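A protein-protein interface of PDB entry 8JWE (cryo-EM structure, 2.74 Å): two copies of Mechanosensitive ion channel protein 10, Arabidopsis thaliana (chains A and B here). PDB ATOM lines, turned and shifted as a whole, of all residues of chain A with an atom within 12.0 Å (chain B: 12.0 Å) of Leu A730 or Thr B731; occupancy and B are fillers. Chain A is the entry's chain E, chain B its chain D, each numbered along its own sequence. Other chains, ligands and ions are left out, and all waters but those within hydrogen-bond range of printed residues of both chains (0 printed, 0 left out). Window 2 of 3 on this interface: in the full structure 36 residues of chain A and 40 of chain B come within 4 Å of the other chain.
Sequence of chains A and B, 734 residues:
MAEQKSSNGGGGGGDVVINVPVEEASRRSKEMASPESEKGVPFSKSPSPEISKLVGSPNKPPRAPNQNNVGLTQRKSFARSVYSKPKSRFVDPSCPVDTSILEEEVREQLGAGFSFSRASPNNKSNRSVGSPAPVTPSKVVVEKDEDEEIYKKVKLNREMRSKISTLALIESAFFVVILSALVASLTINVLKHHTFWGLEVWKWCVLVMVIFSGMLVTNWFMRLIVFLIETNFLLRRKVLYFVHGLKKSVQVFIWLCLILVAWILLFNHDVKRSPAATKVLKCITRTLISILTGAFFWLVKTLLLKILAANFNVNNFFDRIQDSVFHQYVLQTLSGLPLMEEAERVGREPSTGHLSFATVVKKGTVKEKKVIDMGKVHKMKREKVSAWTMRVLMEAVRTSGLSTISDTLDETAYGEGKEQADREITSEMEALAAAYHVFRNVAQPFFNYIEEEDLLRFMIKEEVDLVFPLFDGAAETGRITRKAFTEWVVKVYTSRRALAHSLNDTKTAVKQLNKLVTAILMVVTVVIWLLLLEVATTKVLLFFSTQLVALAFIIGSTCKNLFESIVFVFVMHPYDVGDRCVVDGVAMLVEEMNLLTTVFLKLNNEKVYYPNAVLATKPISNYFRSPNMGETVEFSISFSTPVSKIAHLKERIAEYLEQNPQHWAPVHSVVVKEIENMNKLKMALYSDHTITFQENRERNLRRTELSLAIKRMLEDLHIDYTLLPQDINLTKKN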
ATOM      1  N   PRO A 725      10.302 -32.912  13.500  1.00  0.00           N
ATOM      2  CA  PRO A 725      11.173 -32.382  12.442  1.00  0.00           C
ATOM      3  C   PRO A 725      10.471 -32.118  11.120  1.00  0.00           C
ATOM      4  O   PRO A 725       9.441 -32.693  10.808  1.00  0.00           O
ATOM      5  CB  PRO A 725      12.206 -33.485  12.285  1.00  0.00           C
ATOM      6  CG  PRO A 725      12.153 -34.145  13.350  1.00  0.00           C
ATOM      7  CD  PRO A 725      10.830 -34.179  13.950  1.00  0.00           C
ATOM      8  N   GLN A 726      11.065 -31.268  10.320  1.00  0.00           N
ATOM      9  CA  GLN A 726      10.509 -30.859   9.048  1.00  0.00           C
ATOM     10  C   GLN A 726      11.496 -31.075   7.913  1.00  0.00           C
ATOM     11  O   GLN A 726      12.619 -30.630   7.992  1.00  0.00           O
ATOM     12  CB  GLN A 726      10.073 -29.411   9.127  1.00  0.00           C
ATOM     13  CG  GLN A 726       9.468 -28.877   7.905  1.00  0.00           C
ATOM     14  CD  GLN A 726       8.235 -29.539   7.515  1.00  0.00           C
ATOM     15  OE1 GLN A 726       8.179 -30.259   6.586  1.00  0.00           O
ATOM     16  NE2 GLN A 726       7.235 -29.311   8.248  1.00  0.00           N
ATOM     17  N   ASP A 727      11.074 -31.745   6.867  1.00  0.00           N
ATOM     18  CA  ASP A 727      11.822 -31.850   5.628  1.00  0.00           C
ATOM     19  C   ASP A 727      11.600 -30.689   4.695  1.00  0.00           C
ATOM     20  O   ASP A 727      10.472 -30.314   4.443  1.00  0.00           O
ATOM     21  CB  ASP A 727      11.413 -33.056   4.850  1.00  0.00           C
ATOM     22  CG  ASP A 727      11.920 -34.294   5.389  1.00  0.00           C
ATOM     23  OD1 ASP A 727      12.972 -34.310   6.013  1.00  0.00           O
ATOM     24  OD2 ASP A 727      11.265 -35.315   5.152  1.00  0.00           O
ATOM     25  N   ILE A 728      12.671 -30.203   4.096  1.00  0.00           N
ATOM     26  CA  ILE A 728      12.649 -29.087   3.172  1.00  0.00           C
ATOM     27  C   ILE A 728      13.245 -29.548   1.865  1.00  0.00           C
ATOM     28  O   ILE A 728      14.367 -30.031   1.838  1.00  0.00           O
ATOM     29  CB  ILE A 728      13.413 -27.883   3.739  1.00  0.00           C
ATOM     30  CG1 ILE A 728      12.743 -27.346   5.002  1.00  0.00           C
ATOM     31  CG2 ILE A 728      13.588 -26.845   2.762  1.00  0.00           C
ATOM     32  CD1 ILE A 728      11.367 -26.984   4.909  1.00  0.00           C
ATOM     33  N   ASN A 729      12.491 -29.448   0.794  1.00  0.00           N
ATOM     34  CA  ASN A 729      12.992 -29.655  -0.551  1.00  0.00           C
ATOM     35  C   ASN A 729      13.288 -28.324  -1.174  1.00  0.00           C
ATOM     36  O   ASN A 729      12.377 -27.586  -1.497  1.00  0.00           O
ATOM     37  CB  ASN A 729      11.988 -30.350  -1.433  1.00  0.00           C
ATOM     38  CG  ASN A 729      11.829 -31.751  -1.109  1.00  0.00           C
ATOM     39  OD1 ASN A 729      12.776 -32.486  -1.076  1.00  0.00           O
ATOM     40  ND2 ASN A 729      10.610 -32.141  -0.776  1.00  0.00           N
ATOM     41  N   LEU A 730      14.531 -28.058  -1.422  1.00  0.00           N
ATOM     42  CA  LEU A 730      14.933 -26.737  -1.835  1.00  0.00           C
ATOM     43  C   LEU A 730      15.063 -26.678  -3.333  1.00  0.00           C
ATOM     44  O   LEU A 730      15.850 -27.389  -3.923  1.00  0.00           O
ATOM     45  CB  LEU A 730      16.248 -26.396  -1.183  1.00  0.00           C
ATOM     46  CG  LEU A 730      16.648 -24.986  -1.041  1.00  0.00           C
ATOM     47  CD1 LEU A 730      15.644 -24.419  -0.153  1.00  0.00           C
ATOM     48  CD2 LEU A 730      17.926 -25.041  -0.347  1.00  0.00           C
ATOM     49  N   THR A 731      14.264 -25.843  -3.951  1.00  0.00           N
ATOM     50  CA  THR A 731      14.232 -25.768  -5.400  1.00  0.00           C
ATOM     51  C   THR A 731      15.106 -24.622  -5.915  1.00  0.00           C
ATOM     52  O   THR A 731      15.001 -23.476  -5.487  1.00  0.00           O
ATOM     53  CB  THR A 731      12.832 -25.564  -5.930  1.00  0.00           C
ATOM     54  OG1 THR A 731      11.992 -26.666  -5.582  1.00  0.00           O
ATOM     55  CG2 THR A 731      12.886 -25.386  -7.397  1.00  0.00           C
ATOM     56  N   ASP B 727      13.895 -28.311  14.143  1.00  0.00           N
ATOM     57  CA  ASP B 727      14.827 -29.041  13.302  1.00  0.00           C
ATOM     58  C   ASP B 727      14.435 -29.057  11.848  1.00  0.00           C
ATOM     59  O   ASP B 727      13.301 -29.345  11.524  1.00  0.00           O
ATOM     60  CB  ASP B 727      14.901 -30.478  13.698  1.00  0.00           C
ATOM     61  CG  ASP B 727      15.646 -30.709  14.912  1.00  0.00           C
ATOM     62  OD1 ASP B 727      16.548 -29.950  15.236  1.00  0.00           O
ATOM     63  OD2 ASP B 727      15.350 -31.714  15.564  1.00  0.00           O
ATOM     64  N   ILE B 728      15.405 -28.859  10.976  1.00  0.00           N
ATOM     65  CA  ILE B 728      15.214 -28.835   9.540  1.00  0.00           C
ATOM     66  C   ILE B 728      16.110 -29.883   8.929  1.00  0.00           C
ATOM     67  O   ILE B 728      17.313 -29.862   9.144  1.00  0.00           O
ATOM     68  CB  ILE B 728      15.509 -27.444   8.965  1.00  0.00           C
ATOM     69  CG1 ILE B 728      14.527 -26.402   9.499  1.00  0.00           C
ATOM     70  CG2 ILE B 728      15.535 -27.447   7.528  1.00  0.00           C
ATOM     71  CD1 ILE B 728      13.137 -26.662   9.316  1.00  0.00           C
ATOM     72  N   ASN B 729      15.535 -30.821   8.211  1.00  0.00           N
ATOM     73  CA  ASN B 729      16.277 -31.766   7.400  1.00  0.00           C
ATOM     74  C   ASN B 729      16.279 -31.293   5.976  1.00  0.00           C
ATOM     75  O   ASN B 729      15.260 -31.342   5.316  1.00  0.00           O
ATOM     76  CB  ASN B 729      15.660 -33.139   7.416  1.00  0.00           C
ATOM     77  CG  ASN B 729      15.853 -33.828   8.673  1.00  0.00           C
ATOM     78  OD1 ASN B 729      16.952 -33.976   9.131  1.00  0.00           O
ATOM     79  ND2 ASN B 729      14.757 -34.203   9.311  1.00  0.00           N
ATOM     80  N   LEU B 730      17.420 -30.928   5.483  1.00  0.00           N
ATOM     81  CA  LEU B 730      17.492 -30.279   4.198  1.00  0.00           C
ATOM     82  C   LEU B 730      17.831 -31.282   3.129  1.00  0.00           C
ATOM     83  O   LEU B 730      18.870 -31.911   3.165  1.00  0.00           O
ATOM     84  CB  LEU B 730      18.540 -29.198   4.252  1.00  0.00           C
ATOM     85  CG  LEU B 730      18.500 -28.094   3.278  1.00  0.00           C
ATOM     86  CD1 LEU B 730      17.251 -27.406   3.571  1.00  0.00           C
ATOM     87  CD2 LEU B 730      19.618 -27.241   3.652  1.00  0.00           C
ATOM     88  N   THR B 731      16.938 -31.448   2.187  1.00  0.00           N
ATOM     89  CA  THR B 731      17.111 -32.455   1.156  1.00  0.00           C
ATOM     90  C   THR B 731      17.696 -31.845  -0.121  1.00  0.00           C
ATOM     91  O   THR B 731      17.206 -30.854  -0.656  1.00  0.00           O
ATOM     92  CB  THR B 731      15.811 -33.135   0.796  1.00  0.00           C
ATOM     93  OG1 THR B 731      15.270 -33.827   1.924  1.00  0.00           O
ATOM     94  CG2 THR B 731      16.039 -34.063  -0.331  1.00  0.00           C
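Ile A728 touches its own counterpart, Ile B728. Ile A728 touches Asn B729, but with the chains exchanged Asn A729 does not touch Ile B728 (7.7 Å). Ile A728 touches Thr B731, but with the chains exchanged Thr A731 does not touch Ile B728 (11.7 Å). Leu A730 touches Thr B731, but with the chains exchanged Thr A731 does not touch Leu B730 (8.2 Å). Of the 12 pairs that touch across the chains among the printed residues, 1 has its exchanged pair printed and touching as well.
O of Asp B727 lies within hydrogen-bond range of N of Gln A726, at 3.2 Å. O of Gln A726 sits at hydrogen-bond distance from N of Asn B729 (2.9 Å). O of Asn B729 sits at hydrogen-bond distance from N of Ile A728 (3.1 Å). The backbone NH of Thr B731 lies within hydrogen-bond range of the backbone carbonyl oxygen of Ile A728, at 3.0 Å.
Printed residues of chain B within 4 Å of Pro A725: Asp B727 (3.8 Å) and Asn B729 (3.98 Å). Printed residues of chain B within 4 Å of Gln A726: Asp B727, Ile B728 and Asn B729. Of the printed residues of chain B, Asp A727 touches Asn B729. Printed residues of chain B within 4 Å of Leu A730: Thr B731 (3.9 Å). No residue of chain B comes within 4 Å of Thr A731. Printed residues of chain A within 4 Å of Asp B727: Pro A725 (3.8 Å) and Gln A726 (3.2 Å). Printed residues of chain A within 4 Å of Ile B728: Gln A726 (3.5 Å) and Ile A728 (3.8 Å). Printed residues of chain A within 4 Å of Asn B729: Pro A725 (3.98 Å), Gln A726 (2.9 Å), Asp A727 (3.3 Å) and Ile A728 (3.1 Å). Of the printed residues of chain A, Leu B730 touches Ile A728. Thr B731 touches three residues of chain A. The nearest residue of chain A that does not touch Thr B731 is Asp A727 (4.7 Å).
Pro A725 touches Asp B727 (CA to O, 3.8 Å). Asn B729 touches Pro A725. Ile B728 touches Gln A726. CB of Asn B729 touches OD1 of Asp A727, 3.3 Å away. Ile A728 touches Ile B728 (CG1 to CG2, 3.8 Å). Ile A728 touches Leu B730 (CG2 to CD1, 3.8 Å). Thr B731 touches Asn A729. Leu A730 touches Thr B731 (N to O, 3.9 Å).
Hydrophobic or aromatic side chains of chain A that line the printed part of chain B: Pro A725 and Ile A728. Hydrophobic or aromatic side chains of chain B that line the printed part of chain A: Ile B728 and Leu B730. Among the printed residues, 12 pairs touch across the chains.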
